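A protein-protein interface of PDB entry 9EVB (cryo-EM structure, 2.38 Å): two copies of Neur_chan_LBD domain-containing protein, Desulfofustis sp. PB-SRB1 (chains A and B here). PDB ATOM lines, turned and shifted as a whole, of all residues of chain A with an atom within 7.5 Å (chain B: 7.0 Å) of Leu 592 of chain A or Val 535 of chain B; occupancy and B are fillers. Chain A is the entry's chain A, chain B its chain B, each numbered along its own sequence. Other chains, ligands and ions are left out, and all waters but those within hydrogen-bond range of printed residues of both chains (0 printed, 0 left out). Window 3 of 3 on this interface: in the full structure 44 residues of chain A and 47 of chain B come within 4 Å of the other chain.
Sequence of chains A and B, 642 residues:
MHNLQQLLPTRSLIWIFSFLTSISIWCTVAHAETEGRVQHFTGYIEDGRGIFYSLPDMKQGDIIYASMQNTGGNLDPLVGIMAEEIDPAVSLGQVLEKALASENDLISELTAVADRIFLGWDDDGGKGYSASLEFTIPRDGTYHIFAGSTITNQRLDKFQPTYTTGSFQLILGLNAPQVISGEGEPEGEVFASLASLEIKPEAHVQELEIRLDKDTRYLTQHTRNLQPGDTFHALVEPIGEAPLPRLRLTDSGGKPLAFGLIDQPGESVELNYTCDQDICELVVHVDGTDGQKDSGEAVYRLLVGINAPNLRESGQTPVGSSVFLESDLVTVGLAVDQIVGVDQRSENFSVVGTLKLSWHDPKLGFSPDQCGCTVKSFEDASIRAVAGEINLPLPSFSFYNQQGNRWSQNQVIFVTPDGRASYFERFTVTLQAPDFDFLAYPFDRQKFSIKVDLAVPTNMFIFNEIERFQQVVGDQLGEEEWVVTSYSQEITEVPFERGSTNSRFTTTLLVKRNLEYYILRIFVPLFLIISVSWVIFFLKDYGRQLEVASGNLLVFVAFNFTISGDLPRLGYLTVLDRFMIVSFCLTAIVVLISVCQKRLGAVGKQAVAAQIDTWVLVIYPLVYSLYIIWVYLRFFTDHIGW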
ATOM      1  N   LEU A 546      29.140 -11.365  -3.917  1.00  0.00           N
ATOM      2  CA  LEU A 546      28.056 -11.976  -4.687  1.00  0.00           C
ATOM      3  C   LEU A 546      28.578 -12.662  -5.940  1.00  0.00           C
ATOM      4  O   LEU A 546      28.185 -13.795  -6.254  1.00  0.00           O
ATOM      5  CB  LEU A 546      27.029 -10.916  -5.079  1.00  0.00           C
ATOM      6  CG  LEU A 546      25.708 -11.316  -5.754  1.00  0.00           C
ATOM      7  CD1 LEU A 546      25.196 -12.611  -5.130  1.00  0.00           C
ATOM      8  CD2 LEU A 546      24.699 -10.163  -5.666  1.00  0.00           C
ATOM      9  N   ALA A 549      30.512 -15.815  -5.043  1.00  0.00           N
ATOM     10  CA  ALA A 549      29.598 -16.870  -4.607  1.00  0.00           C
ATOM     11  C   ALA A 549      28.921 -17.531  -5.796  1.00  0.00           C
ATOM     12  O   ALA A 549      28.783 -18.768  -5.850  1.00  0.00           O
ATOM     13  CB  ALA A 549      28.536 -16.296  -3.666  1.00  0.00           C
ATOM     14  N   CYS A 585      23.330 -27.396  -0.779  1.00  0.00           N
ATOM     15  CA  CYS A 585      22.334 -26.525  -0.169  1.00  0.00           C
ATOM     16  C   CYS A 585      23.004 -25.364   0.556  1.00  0.00           C
ATOM     17  O   CYS A 585      22.573 -24.207   0.435  1.00  0.00           O
ATOM     18  CB  CYS A 585      21.433 -27.316   0.777  1.00  0.00           C
ATOM     19  SG  CYS A 585      20.402 -28.528  -0.080  1.00  0.00           S
ATOM     20  N   LEU A 586      24.081 -25.650   1.290  1.00  0.00           N
ATOM     21  CA  LEU A 586      24.792 -24.576   1.974  1.00  0.00           C
ATOM     22  C   LEU A 586      25.424 -23.591   0.985  1.00  0.00           C
ATOM     23  O   LEU A 586      25.299 -22.370   1.164  1.00  0.00           O
ATOM     24  CB  LEU A 586      25.813 -25.178   2.932  1.00  0.00           C
ATOM     25  CG  LEU A 586      25.177 -25.913   4.117  1.00  0.00           C
ATOM     26  CD1 LEU A 586      26.235 -26.494   5.030  1.00  0.00           C
ATOM     27  CD2 LEU A 586      24.250 -24.987   4.897  1.00  0.00           C
ATOM     28  N   THR A 587      25.995 -24.102  -0.112  1.00  0.00           N
ATOM     29  CA  THR A 587      26.570 -23.225  -1.129  1.00  0.00           C
ATOM     30  C   THR A 587      25.519 -22.293  -1.734  1.00  0.00           C
ATOM     31  O   THR A 587      25.805 -21.120  -2.000  1.00  0.00           O
ATOM     32  CB  THR A 587      27.243 -24.068  -2.213  1.00  0.00           C
ATOM     33  OG1 THR A 587      28.213 -24.931  -1.608  1.00  0.00           O
ATOM     34  CG2 THR A 587      27.963 -23.181  -3.210  1.00  0.00           C
ATOM     35  N   ALA A 588      24.296 -22.783  -1.951  1.00  0.00           N
ATOM     36  CA  ALA A 588      23.259 -21.906  -2.503  1.00  0.00           C
ATOM     37  C   ALA A 588      22.765 -20.887  -1.469  1.00  0.00           C
ATOM     38  O   ALA A 588      22.490 -19.720  -1.813  1.00  0.00           O
ATOM     39  CB  ALA A 588      22.104 -22.740  -3.052  1.00  0.00           C
ATOM     40  N   ILE A 589      22.661 -21.306  -0.204  1.00  0.00           N
ATOM     41  CA  ILE A 589      22.285 -20.367   0.847  1.00  0.00           C
ATOM     42  C   ILE A 589      23.314 -19.244   0.959  1.00  0.00           C
ATOM     43  O   ILE A 589      22.976 -18.112   1.334  1.00  0.00           O
ATOM     44  CB  ILE A 589      22.094 -21.110   2.185  1.00  0.00           C
ATOM     45  CG1 ILE A 589      20.902 -22.067   2.129  1.00  0.00           C
ATOM     46  CG2 ILE A 589      21.800 -20.129   3.272  1.00  0.00           C
ATOM     47  CD1 ILE A 589      20.747 -22.912   3.396  1.00  0.00           C
ATOM     48  N   VAL A 590      24.582 -19.536   0.655  1.00  0.00           N
ATOM     49  CA  VAL A 590      25.596 -18.479   0.652  1.00  0.00           C
ATOM     50  C   VAL A 590      25.232 -17.384  -0.349  1.00  0.00           C
ATOM     51  O   VAL A 590      25.319 -16.185  -0.046  1.00  0.00           O
ATOM     52  CB  VAL A 590      26.994 -19.059   0.371  1.00  0.00           C
ATOM     53  CG1 VAL A 590      27.979 -17.933   0.291  1.00  0.00           C
ATOM     54  CG2 VAL A 590      27.424 -19.864   1.551  1.00  0.00           C
ATOM     55  N   VAL A 591      24.809 -17.776  -1.554  1.00  0.00           N
ATOM     56  CA  VAL A 591      24.417 -16.787  -2.557  1.00  0.00           C
ATOM     57  C   VAL A 591      23.209 -15.985  -2.087  1.00  0.00           C
ATOM     58  O   VAL A 591      23.135 -14.761  -2.280  1.00  0.00           O
ATOM     59  CB  VAL A 591      24.149 -17.480  -3.905  1.00  0.00           C
ATOM     60  CG1 VAL A 591      23.878 -16.457  -4.982  1.00  0.00           C
ATOM     61  CG2 VAL A 591      25.332 -18.352  -4.292  1.00  0.00           C
ATOM     62  N   LEU A 592      22.243 -16.664  -1.468  1.00  0.00           N
ATOM     63  CA  LEU A 592      21.054 -15.958  -0.993  1.00  0.00           C
ATOM     64  C   LEU A 592      21.411 -14.890   0.050  1.00  0.00           C
ATOM     65  O   LEU A 592      20.986 -13.726  -0.066  1.00  0.00           O
ATOM     66  CB  LEU A 592      20.042 -16.959  -0.442  1.00  0.00           C
ATOM     67  CG  LEU A 592      19.378 -17.937  -1.414  1.00  0.00           C
ATOM     68  CD1 LEU A 592      18.373 -18.791  -0.665  1.00  0.00           C
ATOM     69  CD2 LEU A 592      18.700 -17.202  -2.557  1.00  0.00           C
ATOM     70  N   ILE A 593      22.261 -15.254   1.019  1.00  0.00           N
ATOM     71  CA  ILE A 593      22.689 -14.309   2.054  1.00  0.00           C
ATOM     72  C   ILE A 593      23.473 -13.154   1.441  1.00  0.00           C
ATOM     73  O   ILE A 593      23.494 -12.029   1.962  1.00  0.00           O
ATOM     74  CB  ILE A 593      23.527 -15.053   3.109  1.00  0.00           C
ATOM     75  CG1 ILE A 593      22.690 -16.115   3.824  1.00  0.00           C
ATOM     76  CG2 ILE A 593      24.102 -14.085   4.115  1.00  0.00           C
ATOM     77  CD1 ILE A 593      23.515 -17.035   4.725  1.00  0.00           C
ATOM     78  N   SER A 594      24.219 -13.445   0.377  1.00  0.00           N
ATOM     79  CA  SER A 594      25.029 -12.436  -0.301  1.00  0.00           C
ATOM     80  C   SER A 594      24.137 -11.397  -0.972  1.00  0.00           C
ATOM     81  O   SER A 594      24.426 -10.192  -0.948  1.00  0.00           O
ATOM     82  CB  SER A 594      25.956 -13.093  -1.323  1.00  0.00           C
ATOM     83  OG  SER A 594      26.933 -13.914  -0.702  1.00  0.00           O
ATOM     84  N   VAL A 595      23.032 -11.855  -1.561  1.00  0.00           N
ATOM     85  CA  VAL A 595      22.077 -10.933  -2.171  1.00  0.00           C
ATOM     86  C   VAL A 595      21.403 -10.076  -1.105  1.00  0.00           C
ATOM     87  O   VAL A 595      21.205  -8.863  -1.278  1.00  0.00           O
ATOM     88  CB  VAL A 595      21.030 -11.708  -2.989  1.00  0.00           C
ATOM     89  CG1 VAL A 595      20.055 -10.746  -3.618  1.00  0.00           C
ATOM     90  CG2 VAL A 595      21.716 -12.478  -4.089  1.00  0.00           C
ATOM     91  N   CYS A 596      21.094 -10.686   0.039  1.00  0.00           N
ATOM     92  CA  CYS A 596      20.484  -9.925   1.126  1.00  0.00           C
ATOM     93  C   CYS A 596      21.425  -8.850   1.663  1.00  0.00           C
ATOM     94  O   CYS A 596      21.016  -7.702   1.881  1.00  0.00           O
ATOM     95  CB  CYS A 596      20.056 -10.880   2.231  1.00  0.00           C
ATOM     96  SG  CYS A 596      19.187 -10.086   3.567  1.00  0.00           S
ATOM     97  N   GLN A 597      22.695  -9.196   1.824  1.00  0.00           N
ATOM     98  CA  GLN A 597      23.691  -8.261   2.327  1.00  0.00           C
ATOM     99  C   GLN A 597      23.962  -7.139   1.330  1.00  0.00           C
ATOM    100  O   GLN A 597      24.190  -5.989   1.726  1.00  0.00           O
ATOM    101  CB  GLN A 597      24.953  -9.044   2.652  1.00  0.00           C
ATOM    102  CG  GLN A 597      24.979  -9.891   3.926  1.00  0.00           C
ATOM    103  CD  GLN A 597      26.372 -10.356   4.240  1.00  0.00           C
ATOM    104  OE1 GLN A 597      27.059 -10.961   3.413  1.00  0.00           O
ATOM    105  NE2 GLN A 597      26.797 -10.086   5.468  1.00  0.00           N
ATOM    106  N   LYS A 598      23.938  -7.452   0.030  1.00  0.00           N
ATOM    107  CA  LYS A 598      24.078  -6.417  -0.990  1.00  0.00           C
ATOM    108  C   LYS A 598      22.931  -5.414  -0.909  1.00  0.00           C
ATOM    109  O   LYS A 598      23.153  -4.195  -0.962  1.00  0.00           O
ATOM    110  CB  LYS A 598      24.136  -7.054  -2.380  1.00  0.00           C
ATOM    111  CG  LYS A 598      24.189  -6.056  -3.532  1.00  0.00           C
ATOM    112  CD  LYS A 598      25.460  -5.224  -3.486  1.00  0.00           C
ATOM    113  CE  LYS A 598      25.636  -4.386  -4.742  1.00  0.00           C
ATOM    114  NZ  LYS A 598      24.480  -3.476  -4.956  1.00  0.00           N
ATOM    115  N   ARG A 599      21.695  -5.907  -0.772  1.00  0.00           N
ATOM    116  CA  ARG A 599      20.563  -4.989  -0.642  1.00  0.00           C
ATOM    117  C   ARG A 599      20.681  -4.143   0.620  1.00  0.00           C
ATOM    118  O   ARG A 599      20.447  -2.925   0.595  1.00  0.00           O
ATOM    119  CB  ARG A 599      19.249  -5.769  -0.637  1.00  0.00           C
ATOM    120  CG  ARG A 599      18.029  -4.871  -0.603  1.00  0.00           C
ATOM    121  CD  ARG A 599      18.192  -3.732  -1.598  1.00  0.00           C
ATOM    122  NE  ARG A 599      17.043  -2.836  -1.610  1.00  0.00           N
ATOM    123  CZ  ARG A 599      17.042  -1.650  -2.203  1.00  0.00           C
ATOM    124  NH1 ARG A 599      18.039  -1.269  -2.988  1.00  0.00           N
ATOM    125  NH2 ARG A 599      16.036  -0.814  -1.976  1.00  0.00           N
ATOM    126  N   LEU B 528      16.055 -24.362  -4.503  1.00  0.00           N
ATOM    127  CA  LEU B 528      17.037 -23.329  -4.174  1.00  0.00           C
ATOM    128  C   LEU B 528      17.445 -22.525  -5.410  1.00  0.00           C
ATOM    129  O   LEU B 528      17.601 -21.297  -5.347  1.00  0.00           O
ATOM    130  CB  LEU B 528      18.252 -23.970  -3.502  1.00  0.00           C
ATOM    131  CG  LEU B 528      17.981 -24.487  -2.083  1.00  0.00           C
ATOM    132  CD1 LEU B 528      19.201 -25.178  -1.497  1.00  0.00           C
ATOM    133  CD2 LEU B 528      17.521 -23.357  -1.171  1.00  0.00           C
ATOM    134  N   ILE B 529      17.607 -23.198  -6.551  1.00  0.00           N
ATOM    135  CA  ILE B 529      17.975 -22.501  -7.786  1.00  0.00           C
ATOM    136  C   ILE B 529      16.873 -21.517  -8.199  1.00  0.00           C
ATOM    137  O   ILE B 529      17.146 -20.346  -8.539  1.00  0.00           O
ATOM    138  CB  ILE B 529      18.286 -23.543  -8.881  1.00  0.00           C
ATOM    139  CG1 ILE B 529      19.566 -24.322  -8.555  1.00  0.00           C
ATOM    140  CG2 ILE B 529      18.428 -22.897 -10.246  1.00  0.00           C
ATOM    141  CD1 ILE B 529      19.897 -25.450  -9.541  1.00  0.00           C
ATOM    142  N   ILE B 530      15.617 -21.963  -8.122  1.00  0.00           N
ATOM    143  CA  ILE B 530      14.481 -21.097  -8.415  1.00  0.00           C
ATOM    144  C   ILE B 530      14.439 -19.901  -7.461  1.00  0.00           C
ATOM    145  O   ILE B 530      14.186 -18.765  -7.884  1.00  0.00           O
ATOM    146  CB  ILE B 530      13.178 -21.918  -8.373  1.00  0.00           C
ATOM    147  CG1 ILE B 530      13.166 -22.963  -9.493  1.00  0.00           C
ATOM    148  CG2 ILE B 530      11.982 -21.015  -8.473  1.00  0.00           C
ATOM    149  CD1 ILE B 530      11.939 -23.859  -9.497  1.00  0.00           C
ATOM    150  N   SER B 531      14.670 -20.145  -6.161  1.00  0.00           N
ATOM    151  CA  SER B 531      14.741 -19.064  -5.180  1.00  0.00           C
ATOM    152  C   SER B 531      15.822 -18.048  -5.532  1.00  0.00           C
ATOM    153  O   SER B 531      15.666 -16.850  -5.273  1.00  0.00           O
ATOM    154  CB  SER B 531      15.008 -19.630  -3.784  1.00  0.00           C
ATOM    155  OG  SER B 531      14.067 -20.617  -3.412  1.00  0.00           O
ATOM    156  N   VAL B 532      16.937 -18.512  -6.087  1.00  0.00           N
ATOM    157  CA  VAL B 532      18.030 -17.609  -6.450  1.00  0.00           C
ATOM    158  C   VAL B 532      17.556 -16.663  -7.542  1.00  0.00           C
ATOM    159  O   VAL B 532      17.771 -15.445  -7.473  1.00  0.00           O
ATOM    160  CB  VAL B 532      19.298 -18.368  -6.883  1.00  0.00           C
ATOM    161  CG1 VAL B 532      20.356 -17.380  -7.360  1.00  0.00           C
ATOM    162  CG2 VAL B 532      19.864 -19.099  -5.701  1.00  0.00           C
ATOM    163  N   SER B 533      16.874 -17.202  -8.558  1.00  0.00           N
ATOM    164  CA  SER B 533      16.366 -16.278  -9.576  1.00  0.00           C
ATOM    165  C   SER B 533      15.189 -15.437  -9.074  1.00  0.00           C
ATOM    166  O   SER B 533      14.906 -14.386  -9.659  1.00  0.00           O
ATOM    167  CB  SER B 533      15.938 -17.015 -10.844  1.00  0.00           C
ATOM    168  OG  SER B 533      16.976 -17.813 -11.369  1.00  0.00           O
ATOM    169  N   TRP B 534      14.494 -15.869  -8.013  1.00  0.00           N
ATOM    170  CA  TRP B 534      13.390 -15.059  -7.493  1.00  0.00           C
ATOM    171  C   TRP B 534      13.889 -13.890  -6.649  1.00  0.00           C
ATOM    172  O   TRP B 534      13.330 -12.790  -6.711  1.00  0.00           O
ATOM    173  CB  TRP B 534      12.431 -15.919  -6.664  1.00  0.00           C
ATOM    174  CG  TRP B 534      11.340 -15.128  -5.989  1.00  0.00           C
ATOM    175  CD1 TRP B 534      10.198 -14.643  -6.551  1.00  0.00           C
ATOM    176  CD2 TRP B 534      11.293 -14.757  -4.604  1.00  0.00           C
ATOM    177  NE1 TRP B 534       9.464 -13.954  -5.611  1.00  0.00           N
ATOM    178  CE2 TRP B 534      10.100 -14.038  -4.401  1.00  0.00           C
ATOM    179  CE3 TRP B 534      12.154 -14.956  -3.516  1.00  0.00           C
ATOM    180  CZ2 TRP B 534       9.747 -13.513  -3.160  1.00  0.00           C
ATOM    181  CZ3 TRP B 534      11.802 -14.435  -2.288  1.00  0.00           C
ATOM    182  CH2 TRP B 534      10.607 -13.727  -2.116  1.00  0.00           C
ATOM    183  N   VAL B 535      14.932 -14.108  -5.849  1.00  0.00           N
ATOM    184  CA  VAL B 535      15.320 -13.116  -4.855  1.00  0.00           C
ATOM    185  C   VAL B 535      15.971 -11.882  -5.473  1.00  0.00           C
ATOM    186  O   VAL B 535      15.998 -10.820  -4.841  1.00  0.00           O
ATOM    187  CB  VAL B 535      16.257 -13.760  -3.813  1.00  0.00           C
ATOM    188  CG1 VAL B 535      17.629 -14.031  -4.421  1.00  0.00           C
ATOM    189  CG2 VAL B 535      16.363 -12.889  -2.564  1.00  0.00           C
ATOM    190  N   ILE B 536      16.479 -11.977  -6.705  1.00  0.00           N
ATOM    191  CA  ILE B 536      17.299 -10.896  -7.252  1.00  0.00           C
ATOM    192  C   ILE B 536      16.497  -9.658  -7.613  1.00  0.00           C
ATOM    193  O   ILE B 536      17.083  -8.600  -7.868  1.00  0.00           O
ATOM    194  CB  ILE B 536      18.075 -11.366  -8.499  1.00  0.00           C
ATOM    195  CG1 ILE B 536      17.104 -11.921  -9.547  1.00  0.00           C
ATOM    196  CG2 ILE B 536      19.095 -12.413  -8.114  1.00  0.00           C
ATOM    197  CD1 ILE B 536      17.762 -12.352 -10.835  1.00  0.00           C
ATOM    198  N   PHE B 537      15.171  -9.761  -7.638  1.00  0.00           N
ATOM    199  CA  PHE B 537      14.292  -8.658  -8.001  1.00  0.00           C
ATOM    200  C   PHE B 537      14.166  -7.622  -6.894  1.00  0.00           C
ATOM    201  O   PHE B 537      13.599  -6.552  -7.134  1.00  0.00           O
ATOM    202  CB  PHE B 537      12.910  -9.182  -8.396  1.00  0.00           C
ATOM    203  CG  PHE B 537      12.843  -9.702  -9.805  1.00  0.00           C
ATOM    204  CD1 PHE B 537      13.221 -11.001 -10.092  1.00  0.00           C
ATOM    205  CD2 PHE B 537      12.426  -8.885 -10.843  1.00  0.00           C
ATOM    206  CE1 PHE B 537      13.193 -11.475 -11.386  1.00  0.00           C
ATOM    207  CE2 PHE B 537      12.399  -9.354 -12.143  1.00  0.00           C
ATOM    208  CZ  PHE B 537      12.746 -10.662 -12.408  1.00  0.00           C
ATOM    209  N   PHE B 538      14.679  -7.907  -5.696  1.00  0.00           N
ATOM    210  CA  PHE B 538      14.758  -6.876  -4.671  1.00  0.00           C
ATOM    211  C   PHE B 538      15.831  -5.835  -4.978  1.00  0.00           C
ATOM    212  O   PHE B 538      15.722  -4.702  -4.496  1.00  0.00           O
ATOM    213  CB  PHE B 538      15.018  -7.505  -3.300  1.00  0.00           C
ATOM    214  CG  PHE B 538      13.820  -8.188  -2.704  1.00  0.00           C
ATOM    215  CD1 PHE B 538      12.841  -7.458  -2.053  1.00  0.00           C
ATOM    216  CD2 PHE B 538      13.682  -9.564  -2.780  1.00  0.00           C
ATOM    217  CE1 PHE B 538      11.742  -8.084  -1.500  1.00  0.00           C
ATOM    218  CE2 PHE B 538      12.584 -10.196  -2.234  1.00  0.00           C
ATOM    219  CZ  PHE B 538      11.619  -9.455  -1.583  1.00  0.00           C
ATOM    220  N   LEU B 539      16.857  -6.186  -5.760  1.00  0.00           N
ATOM    221  CA  LEU B 539      17.907  -5.231  -6.112  1.00  0.00           C
ATOM    222  C   LEU B 539      17.351  -4.099  -6.964  1.00  0.00           C
ATOM    223  O   LEU B 539      16.401  -4.271  -7.733  1.00  0.00           O
ATOM    224  CB  LEU B 539      19.048  -5.904  -6.886  1.00  0.00           C
ATOM    225  CG  LEU B 539      19.772  -7.003  -6.115  1.00  0.00           C
ATOM    226  CD1 LEU B 539      20.729  -7.887  -6.948  1.00  0.00           C
ATOM    227  CD2 LEU B 539      20.449  -6.504  -4.806  1.00  0.00           C
ATOM    228  N   VAL B 548      23.391 -11.660 -12.596  1.00  0.00           N
ATOM    229  CA  VAL B 548      23.078 -12.806 -11.750  1.00  0.00           C
ATOM    230  C   VAL B 548      22.050 -13.707 -12.424  1.00  0.00           C
ATOM    231  O   VAL B 548      22.128 -14.935 -12.321  1.00  0.00           O
ATOM    232  CB  VAL B 548      22.605 -12.357 -10.356  1.00  0.00           C
ATOM    233  CG1 VAL B 548      22.345 -13.574  -9.494  1.00  0.00           C
ATOM    234  CG2 VAL B 548      23.661 -11.512  -9.692  1.00  0.00           C
ATOM    235  N   LEU B 617       7.651 -10.158  -8.213  1.00  0.00           N
ATOM    236  CA  LEU B 617       7.814 -10.758  -6.893  1.00  0.00           C
ATOM    237  C   LEU B 617       6.497 -11.324  -6.378  1.00  0.00           C
ATOM    238  O   LEU B 617       6.479 -12.353  -5.692  1.00  0.00           O
ATOM    239  CB  LEU B 617       8.369  -9.731  -5.906  1.00  0.00           C
ATOM    240  CG  LEU B 617       9.863  -9.421  -5.949  1.00  0.00           C
ATOM    241  CD1 LEU B 617      10.165  -8.190  -5.106  1.00  0.00           C
ATOM    242  CD2 LEU B 617      10.655 -10.624  -5.465  1.00  0.00           C
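CA of Cys 585 of chain A touches CD1 of Leu 528 of chain B (3.7 Å). Leu 592 of chain A touches Val 532 of chain B. Leu 592 of chain A touches Val 535 of chain B (CD2 to CG1, 3.8 Å). Lys 598 of chain A touches Leu 539 of chain B (CG to CD2, 3.98 Å). Arg 599 of chain A touches Phe 538 of chain B (NE to O, 3.7 Å).
Printed residues of chain B within 4 Å of Cys 585 of chain A: Leu 528. Printed residues of chain B within 4 Å of Leu 592 of chain A: Val 532 (3.9 Å) and Val 535 (3.8 Å). Ser 594 of chain A touches none of the printed residues of chain B. Printed residues of chain B within 4 Å of Lys 598 of chain A: Leu 539 (3.98 Å). Printed residues of chain B within 4 Å of Arg 599 of chain A: Phe 538 (3.7 Å). Printed residues of chain A within 4 Å of Val 532 of chain B: Leu 592 (3.9 Å). Trp 534 of chain B touches none of the printed residues of chain A. Of chain A, only Leu 592 (3.8 Å) comes within 4 Å of Val 535 of chain B. Printed residues of chain A within 4 Å of Phe 538 of chain B: Arg 599 (3.7 Å). The nearest residue of chain A that does not touch Val 535 of chain B is Val 595 of chain A (4.2 Å). The nearest printed residue of chain A that does not touch Val 532 of chain B is Val 591 of chain A (4.3 Å).
Hydrophobic or aromatic side chains of chain A within 4 Å of the printed part of chain B: Leu 592. Hydrophobic or aromatic side chains of chain B within 4 Å of the printed part of chain A: Leu 528, Val 532, Val 535 and Leu 539. Among the printed residues, no Asp or Glu carboxylate lies within 4 Å of a Lys or Arg side-chain nitrogen of the other chain.
No position is printed for both chains. Of the 5 pairs that touch across the chains among the printed residues, none has its exchanged pair printed and touching as well.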
